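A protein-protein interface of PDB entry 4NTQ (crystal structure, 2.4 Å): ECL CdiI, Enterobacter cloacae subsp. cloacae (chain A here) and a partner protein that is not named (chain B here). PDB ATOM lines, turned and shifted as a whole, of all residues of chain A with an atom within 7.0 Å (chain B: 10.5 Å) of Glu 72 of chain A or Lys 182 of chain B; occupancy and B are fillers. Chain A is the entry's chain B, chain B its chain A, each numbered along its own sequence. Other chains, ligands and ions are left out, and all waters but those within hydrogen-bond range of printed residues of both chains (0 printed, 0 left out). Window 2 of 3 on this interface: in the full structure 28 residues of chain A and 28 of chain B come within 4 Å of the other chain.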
ATOM      1  N   TYR A  69     -13.959  10.317  15.937  1.00  0.00           N
ATOM      2  CA  TYR A  69     -13.199   9.337  15.191  1.00  0.00           C
ATOM      3  C   TYR A  69     -13.835   9.255  13.838  1.00  0.00           C
ATOM      4  O   TYR A  69     -14.796   9.981  13.568  1.00  0.00           O
ATOM      5  CB  TYR A  69     -13.243   7.991  15.898  1.00  0.00           C
ATOM      6  CG  TYR A  69     -12.607   8.031  17.266  1.00  0.00           C
ATOM      7  CD1 TYR A  69     -13.365   8.310  18.403  1.00  0.00           C
ATOM      8  CD2 TYR A  69     -11.240   7.814  17.424  1.00  0.00           C
ATOM      9  CE1 TYR A  69     -12.779   8.351  19.657  1.00  0.00           C
ATOM     10  CE2 TYR A  69     -10.645   7.853  18.670  1.00  0.00           C
ATOM     11  CZ  TYR A  69     -11.412   8.119  19.781  1.00  0.00           C
ATOM     12  OH  TYR A  69     -10.812   8.161  21.021  1.00  0.00           O
ATOM     13  N   GLU A  70     -13.276   8.404  12.981  1.00  0.00           N
ATOM     14  CA  GLU A  70     -13.911   8.036  11.730  1.00  0.00           C
ATOM     15  C   GLU A  70     -15.368   7.749  12.039  1.00  0.00           C
ATOM     16  O   GLU A  70     -15.666   6.855  12.829  1.00  0.00           O
ATOM     17  CB  GLU A  70     -13.250   6.784  11.163  1.00  0.00           C
ATOM     18  CG  GLU A  70     -13.664   6.445   9.741  1.00  0.00           C
ATOM     19  CD  GLU A  70     -12.966   7.316   8.713  1.00  0.00           C
ATOM     20  OE1 GLU A  70     -11.750   7.556   8.873  1.00  0.00           O
ATOM     21  OE2 GLU A  70     -13.630   7.758   7.749  1.00  0.00           O
ATOM     22  N   PRO A  71     -16.279   8.537  11.455  1.00  0.00           N
ATOM     23  CA  PRO A  71     -17.716   8.409  11.749  1.00  0.00           C
ATOM     24  C   PRO A  71     -18.317   7.005  11.523  1.00  0.00           C
ATOM     25  O   PRO A  71     -19.201   6.613  12.288  1.00  0.00           O
ATOM     26  CB  PRO A  71     -18.356   9.450  10.822  1.00  0.00           C
ATOM     27  CG  PRO A  71     -17.266  10.483  10.630  1.00  0.00           C
ATOM     28  CD  PRO A  71     -15.983   9.699  10.596  1.00  0.00           C
ATOM     29  N   GLU A  72     -17.851   6.261  10.520  1.00  0.00           N
ATOM     30  CA  GLU A  72     -18.367   4.908  10.295  1.00  0.00           C
ATOM     31  C   GLU A  72     -17.773   3.902  11.278  1.00  0.00           C
ATOM     32  O   GLU A  72     -18.320   2.817  11.471  1.00  0.00           O
ATOM     33  CB  GLU A  72     -18.127   4.452   8.847  1.00  0.00           C
ATOM     34  N   LYS A  73     -16.651   4.257  11.896  1.00  0.00           N
ATOM     35  CA  LYS A  73     -16.022   3.356  12.847  1.00  0.00           C
ATOM     36  C   LYS A  73     -16.247   3.833  14.271  1.00  0.00           C
ATOM     37  O   LYS A  73     -15.654   3.318  15.203  1.00  0.00           O
ATOM     38  CB  LYS A  73     -14.531   3.213  12.555  1.00  0.00           C
ATOM     39  N   THR A  74     -17.114   4.821  14.439  1.00  0.00           N
ATOM     40  CA  THR A  74     -17.348   5.411  15.754  1.00  0.00           C
ATOM     41  C   THR A  74     -18.546   4.795  16.475  1.00  0.00           C
ATOM     42  O   THR A  74     -19.621   4.672  15.901  1.00  0.00           O
ATOM     43  CB  THR A  74     -17.570   6.928  15.633  1.00  0.00           C
ATOM     44  OG1 THR A  74     -16.435   7.528  14.999  1.00  0.00           O
ATOM     45  CG2 THR A  74     -17.756   7.549  16.993  1.00  0.00           C
ATOM     46  N   ASN A  75     -18.356   4.413  17.733  1.00  0.00           N
ATOM     47  CA  ASN A  75     -19.459   3.918  18.555  1.00  0.00           C
ATOM     48  C   ASN A  75     -20.169   5.008  19.352  1.00  0.00           C
ATOM     49  O   ASN A  75     -21.379   4.932  19.573  1.00  0.00           O
ATOM     50  CB  ASN A  75     -18.979   2.828  19.511  1.00  0.00           C
ATOM     51  CG  ASN A  75     -18.936   1.477  18.859  1.00  0.00           C
ATOM     52  OD1 ASN A  75     -19.759   1.167  17.990  1.00  0.00           O
ATOM     53  ND2 ASN A  75     -17.970   0.659  19.257  1.00  0.00           N
ATOM     54  N   LEU A  98     -23.730   5.991  18.779  1.00  0.00           N
ATOM     55  CA  LEU A  98     -23.875   5.840  17.337  1.00  0.00           C
ATOM     56  C   LEU A  98     -23.573   4.424  16.853  1.00  0.00           C
ATOM     57  O   LEU A  98     -23.379   4.209  15.651  1.00  0.00           O
ATOM     58  CB  LEU A  98     -22.942   6.819  16.624  1.00  0.00           C
ATOM     59  CG  LEU A  98     -22.873   8.223  17.217  1.00  0.00           C
ATOM     60  CD1 LEU A  98     -21.691   8.967  16.629  1.00  0.00           C
ATOM     61  CD2 LEU A  98     -24.166   8.958  16.943  1.00  0.00           C
ATOM     62  N   GLU A  99     -23.516   3.476  17.787  1.00  0.00           N
ATOM     63  CA  GLU A  99     -23.124   2.105  17.478  1.00  0.00           C
ATOM     64  C   GLU A  99     -24.050   1.521  16.433  1.00  0.00           C
ATOM     65  O   GLU A  99     -23.607   0.808  15.527  1.00  0.00           O
ATOM     66  CB  GLU A  99     -23.126   1.250  18.745  1.00  0.00           C
ATOM     67  N   GLU A 100     -25.332   1.854  16.543  1.00  0.00           N
ATOM     68  CA  GLU A 100     -26.309   1.402  15.564  1.00  0.00           C
ATOM     69  C   GLU A 100     -26.889   2.578  14.785  1.00  0.00           C
ATOM     70  O   GLU A 100     -28.119   2.712  14.652  1.00  0.00           O
ATOM     71  CB  GLU A 100     -27.414   0.563  16.223  1.00  0.00           C
ATOM     72  CG  GLU A 100     -26.929  -0.761  16.814  1.00  0.00           C
ATOM     73  CD  GLU A 100     -26.106  -1.601  15.839  1.00  0.00           C
ATOM     74  OE1 GLU A 100     -26.483  -1.714  14.652  1.00  0.00           O
ATOM     75  OE2 GLU A 100     -25.081  -2.172  16.269  1.00  0.00           O
ATOM     76  N   CYS A 101     -25.990   3.412  14.262  1.00  0.00           N
ATOM     77  CA  CYS A 101     -26.371   4.510  13.382  1.00  0.00           C
ATOM     78  C   CYS A 101     -25.846   4.293  11.958  1.00  0.00           C
ATOM     79  O   CYS A 101     -26.612   4.000  11.027  1.00  0.00           O
ATOM     80  CB  CYS A 101     -25.829   5.832  13.920  1.00  0.00           C
ATOM     81  SG  CYS A 101     -27.074   7.100  14.141  1.00  0.00           S
ATOM     82  N   HIS A 102     -24.531   4.451  11.816  1.00  0.00           N
ATOM     83  CA  HIS A 102     -23.836   4.474  10.525  1.00  0.00           C
ATOM     84  C   HIS A 102     -24.142   5.729   9.706  1.00  0.00           C
ATOM     85  O   HIS A 102     -23.336   6.133   8.860  1.00  0.00           O
ATOM     86  CB  HIS A 102     -24.095   3.200   9.717  1.00  0.00           C
ATOM     87  N   PHE A 104     -24.400   8.749  10.897  1.00  0.00           N
ATOM     88  CA  PHE A 104     -23.848   9.942  11.539  1.00  0.00           C
ATOM     89  C   PHE A 104     -22.771  10.664  10.731  1.00  0.00           C
ATOM     90  O   PHE A 104     -22.004  10.045   9.999  1.00  0.00           O
ATOM     91  CB  PHE A 104     -23.315   9.620  12.943  1.00  0.00           C
ATOM     92  CG  PHE A 104     -22.563  10.764  13.581  1.00  0.00           C
ATOM     93  CD1 PHE A 104     -23.247  11.870  14.072  1.00  0.00           C
ATOM     94  CD2 PHE A 104     -21.175  10.748  13.661  1.00  0.00           C
ATOM     95  CE1 PHE A 104     -22.568  12.935  14.640  1.00  0.00           C
ATOM     96  CE2 PHE A 104     -20.486  11.809  14.234  1.00  0.00           C
ATOM     97  CZ  PHE A 104     -21.185  12.905  14.725  1.00  0.00           C
ATOM     98  N   ARG B 177     -17.553  -3.682  28.223  1.00  0.00           N
ATOM     99  CA  ARG B 177     -16.705  -2.590  27.784  1.00  0.00           C
ATOM    100  C   ARG B 177     -17.135  -2.179  26.391  1.00  0.00           C
ATOM    101  O   ARG B 177     -17.111  -2.985  25.468  1.00  0.00           O
ATOM    102  CB  ARG B 177     -15.240  -3.010  27.745  1.00  0.00           C
ATOM    103  CG  ARG B 177     -14.357  -1.975  27.057  1.00  0.00           C
ATOM    104  CD  ARG B 177     -12.899  -2.400  26.996  1.00  0.00           C
ATOM    105  NE  ARG B 177     -12.035  -1.306  26.555  1.00  0.00           N
ATOM    106  CZ  ARG B 177     -11.638  -1.121  25.299  1.00  0.00           C
ATOM    107  NH1 ARG B 177     -12.026  -1.965  24.347  1.00  0.00           N
ATOM    108  NH2 ARG B 177     -10.851  -0.090  24.996  1.00  0.00           N
ATOM    109  N   ILE B 178     -17.544  -0.933  26.235  1.00  0.00           N
ATOM    110  CA  ILE B 178     -17.830  -0.423  24.905  1.00  0.00           C
ATOM    111  C   ILE B 178     -16.738   0.543  24.497  1.00  0.00           C
ATOM    112  O   ILE B 178     -16.632   1.630  25.057  1.00  0.00           O
ATOM    113  CB  ILE B 178     -19.160   0.324  24.843  1.00  0.00           C
ATOM    114  CG1 ILE B 178     -20.306  -0.573  25.312  1.00  0.00           C
ATOM    115  CG2 ILE B 178     -19.398   0.841  23.430  1.00  0.00           C
ATOM    116  CD1 ILE B 178     -21.635   0.154  25.394  1.00  0.00           C
ATOM    117  N   PRO B 179     -15.915   0.147  23.521  1.00  0.00           N
ATOM    118  CA  PRO B 179     -14.823   1.003  23.053  1.00  0.00           C
ATOM    119  C   PRO B 179     -15.360   2.081  22.129  1.00  0.00           C
ATOM    120  O   PRO B 179     -16.388   1.864  21.491  1.00  0.00           O
ATOM    121  CB  PRO B 179     -13.934   0.036  22.275  1.00  0.00           C
ATOM    122  CG  PRO B 179     -14.879  -1.025  21.799  1.00  0.00           C
ATOM    123  CD  PRO B 179     -15.918  -1.172  22.865  1.00  0.00           C
ATOM    124  N   PRO B 180     -14.674   3.228  22.055  1.00  0.00           N
ATOM    125  CA  PRO B 180     -15.109   4.350  21.213  1.00  0.00           C
ATOM    126  C   PRO B 180     -15.107   4.036  19.720  1.00  0.00           C
ATOM    127  O   PRO B 180     -15.847   4.681  18.976  1.00  0.00           O
ATOM    128  CB  PRO B 180     -14.089   5.453  21.528  1.00  0.00           C
ATOM    129  CG  PRO B 180     -12.925   4.743  22.142  1.00  0.00           C
ATOM    130  CD  PRO B 180     -13.491   3.561  22.863  1.00  0.00           C
ATOM    131  N   GLN B 181     -14.296   3.077  19.289  1.00  0.00           N
ATOM    132  CA  GLN B 181     -14.216   2.715  17.875  1.00  0.00           C
ATOM    133  C   GLN B 181     -14.564   1.250  17.619  1.00  0.00           C
ATOM    134  O   GLN B 181     -14.270   0.389  18.441  1.00  0.00           O
ATOM    135  CB  GLN B 181     -12.819   2.983  17.333  1.00  0.00           C
ATOM    136  CG  GLN B 181     -12.502   4.437  17.103  1.00  0.00           C
ATOM    137  CD  GLN B 181     -11.085   4.633  16.592  1.00  0.00           C
ATOM    138  OE1 GLN B 181     -10.112   4.437  17.326  1.00  0.00           O
ATOM    139  NE2 GLN B 181     -10.965   5.017  15.323  1.00  0.00           N
ATOM    140  N   LYS B 182     -15.174   0.978  16.466  1.00  0.00           N
ATOM    141  CA  LYS B 182     -15.526  -0.386  16.063  1.00  0.00           C
ATOM    142  C   LYS B 182     -14.295  -1.180  15.640  1.00  0.00           C
ATOM    143  O   LYS B 182     -13.226  -0.603  15.405  1.00  0.00           O
ATOM    144  CB  LYS B 182     -16.569  -0.367  14.935  1.00  0.00           C
ATOM    145  CG  LYS B 182     -17.985  -0.045  15.412  1.00  0.00           C
ATOM    146  CD  LYS B 182     -18.940   0.283  14.264  1.00  0.00           C
ATOM    147  CE  LYS B 182     -20.283   0.783  14.803  1.00  0.00           C
ATOM    148  NZ  LYS B 182     -21.153   1.387  13.751  1.00  0.00           N
ATOM    149  N   ALA B 183     -14.447  -2.501  15.549  1.00  0.00           N
ATOM    150  CA  ALA B 183     -13.345  -3.367  15.122  1.00  0.00           C
ATOM    151  C   ALA B 183     -12.726  -2.858  13.831  1.00  0.00           C
ATOM    152  O   ALA B 183     -13.446  -2.403  12.942  1.00  0.00           O
ATOM    153  CB  ALA B 183     -13.814  -4.805  14.968  1.00  0.00           C
ATOM    154  N   PRO B 184     -11.384  -2.916  13.727  1.00  0.00           N
ATOM    155  CA  PRO B 184     -10.424  -3.442  14.707  1.00  0.00           C
ATOM    156  C   PRO B 184      -9.620  -2.353  15.422  1.00  0.00           C
ATOM    157  O   PRO B 184      -8.409  -2.541  15.617  1.00  0.00           O
ATOM    158  CB  PRO B 184      -9.465  -4.241  13.827  1.00  0.00           C
ATOM    159  CG  PRO B 184      -9.493  -3.502  12.474  1.00  0.00           C
ATOM    160  CD  PRO B 184     -10.701  -2.571  12.470  1.00  0.00           C
ATOM    161  N   PHE B 185     -10.268  -1.248  15.797  1.00  0.00           N
ATOM    162  CA  PHE B 185      -9.579  -0.148  16.474  1.00  0.00           C
ATOM    163  C   PHE B 185     -10.103   0.005  17.901  1.00  0.00           C
ATOM    164  O   PHE B 185     -10.253   1.121  18.386  1.00  0.00           O
ATOM    165  CB  PHE B 185      -9.792   1.185  15.742  1.00  0.00           C
ATOM    166  CG  PHE B 185      -9.356   1.196  14.296  1.00  0.00           C
ATOM    167  CD1 PHE B 185      -8.636   0.155  13.740  1.00  0.00           C
ATOM    168  CD2 PHE B 185      -9.672   2.279  13.497  1.00  0.00           C
ATOM    169  CE1 PHE B 185      -8.254   0.184  12.413  1.00  0.00           C
ATOM    170  CE2 PHE B 185      -9.289   2.318  12.170  1.00  0.00           C
ATOM    171  CZ  PHE B 185      -8.578   1.267  11.626  1.00  0.00           C
ATOM    172  N   ASN B 186     -10.367  -1.114  18.568  1.00  0.00           N
ATOM    173  CA  ASN B 186     -11.113  -1.115  19.829  1.00  0.00           C
ATOM    174  C   ASN B 186     -10.273  -1.106  21.104  1.00  0.00           C
ATOM    175  O   ASN B 186     -10.829  -1.064  22.208  1.00  0.00           O
ATOM    176  CB  ASN B 186     -12.060  -2.314  19.869  1.00  0.00           C
ATOM    177  CG  ASN B 186     -12.471  -2.767  18.502  1.00  0.00           C
ATOM    178  OD1 ASN B 186     -11.794  -2.479  17.524  1.00  0.00           O
ATOM    179  ND2 ASN B 186     -13.586  -3.482  18.421  1.00  0.00           N
ATOM    180  N   SER B 187      -8.952  -1.181  20.955  1.00  0.00           N
ATOM    181  CA  SER B 187      -8.048  -1.074  22.091  1.00  0.00           C
ATOM    182  C   SER B 187      -7.642   0.384  22.297  1.00  0.00           C
ATOM    183  O   SER B 187      -6.878   0.713  23.204  1.00  0.00           O
ATOM    184  CB  SER B 187      -6.815  -1.942  21.859  1.00  0.00           C
ATOM    185  OG  SER B 187      -6.268  -1.715  20.569  1.00  0.00           O
ATOM    186  N   HIS B 188      -8.183   1.256  21.455  1.00  0.00           N
ATOM    187  CA  HIS B 188      -7.800   2.654  21.448  1.00  0.00           C
ATOM    188  C   HIS B 188      -8.886   3.542  22.035  1.00  0.00           C
ATOM    189  O   HIS B 188      -9.967   3.666  21.454  1.00  0.00           O
ATOM    190  CB  HIS B 188      -7.478   3.100  20.020  1.00  0.00           C
ATOM    191  N   GLY B 189      -8.603   4.140  23.191  1.00  0.00           N
ATOM    192  CA  GLY B 189      -9.347   5.308  23.636  1.00  0.00           C
ATOM    193  C   GLY B 189     -10.141   5.199  24.922  1.00  0.00           C
ATOM    194  O   GLY B 189     -10.230   4.128  25.513  1.00  0.00           O
ATOM    195  N   GLN B 190     -10.704   6.327  25.361  1.00  0.00           N
ATOM    196  CA  GLN B 190     -11.563   6.350  26.537  1.00  0.00           C
ATOM    197  C   GLN B 190     -12.786   5.522  26.234  1.00  0.00           C
ATOM    198  O   GLN B 190     -13.567   5.863  25.352  1.00  0.00           O
ATOM    199  CB  GLN B 190     -11.991   7.774  26.908  1.00  0.00           C
ATOM    200  CG  GLN B 190     -11.026   8.541  27.813  1.00  0.00           C
ATOM    201  CD  GLN B 190     -11.548   9.933  28.187  1.00  0.00           C
ATOM    202  OE1 GLN B 190     -11.048  10.951  27.699  1.00  0.00           O
ATOM    203  NE2 GLN B 190     -12.557   9.976  29.055  1.00  0.00           N
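N of Asn 75 of chain A sits at hydrogen-bond distance from O of Pro 180 of chain B.
The backbone carbonyl oxygen of Pro 179 of chain B sits at hydrogen-bond distance from the side-chain amide nitrogen of Asn 75 of chain A, 3.0 Å away.
NZ of Lys 182 of chain B is in hydrogen-bond range of O of Glu 99 of chain A, 3.1 Å away.
The backbone NH (N) of Lys 182 of chain B lies within hydrogen-bond range of the backbone carbonyl oxygen (O) of Lys 73 of chain A (2.7 Å).
Of chain B, only Lys 182 comes within 4 Å of Glu 72 of chain A.
Lys 182 of chain B touches just these residues of chain A: Glu 72, Lys 73, Asn 75 and Glu 99.
No residue of chain B comes within 4 Å of Pro 71 of chain A.
No residue of chain B comes within 4 Å of His 102 of chain A.
Of the printed residues of chain B, Thr 74 of chain A touches Pro 180.
Printed residues of chain B within 4 Å of Tyr 69 of chain A: Pro 180 and Gln 181.
Printed residues of chain A within 4 Å of Pro 180 of chain B: Tyr 69 (3.7 Å), Thr 74 (3.6 Å) and Asn 75 (2.8 Å).
Printed residues of chain A within 4 Å of Gln 181 of chain B: Tyr 69, Lys 73 and Asn 75.
Of the printed residues of chain A, Pro 179 of chain B touches Asn 75.
Pro 184 of chain B touches none of the printed residues of chain A.
The nearest residue of chain B that does not touch Glu 72 of chain A is Ala 183 of chain B (7.3 Å).
Among the printed residues, merely in contact across the chains: Tyr 69 of chain A with Pro 180 of chain B (3.7 Å), Tyr 69 of chain A with Gln 181 of chain B (3.3 Å), Glu 72 of chain A with Lys 182 of chain B (3.8 Å), Lys 73 of chain A with Gln 181 of chain B (3.1 Å), Thr 74 of chain A with Pro 180 of chain B (3.6 Å), Asn 75 of chain A with Gln 181 of chain B (3.8 Å) and Asn 75 of chain A with Lys 182 of chain B (3.3 Å).
Hydrophobic or aromatic side chains of chain A within 4 Å of the printed part of chain B: Tyr 69.
Along chain A the printed residues that touch a printed residue of chain B span positions 69 to 99.
Of the 14 printed residues of chain B, 4 touch a printed residue of chain A.
Printed residues of chain B that touch a printed residue of chain A: Pro 179, Pro 180, Gln 181 and Lys 182.
Among the printed residues, no Asp or Glu carboxylate lies within 4 Å of a Lys or Arg side-chain nitrogen of the other chain.
The backbone carbonyl oxygen of Asn 75 of chain A sits at hydrogen-bond distance from the backbone NH of Leu 98 of chain A, at 2.7 Å.
The backbone carbonyl oxygen (O) of Lys 182 of chain B lies close to the side-chain amide oxygen (OD1) of Asn 186 of chain B, at 3.2 Å.
The side-chain hydroxyl of Thr 74 of chain A is in hydrogen-bond range of the backbone carbonyl oxygen of Tyr 69 of chain A (3.3 Å).
The backbone NH of Glu 99 of chain A sits at hydrogen-bond distance from the backbone carbonyl oxygen of Asn 75 of chain A (3.1 Å).
The side-chain amide oxygen (OE1) of Gln 181 of chain B sits close to the backbone carbonyl oxygen (O) of Phe 185 of chain B, at 3.5 Å.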
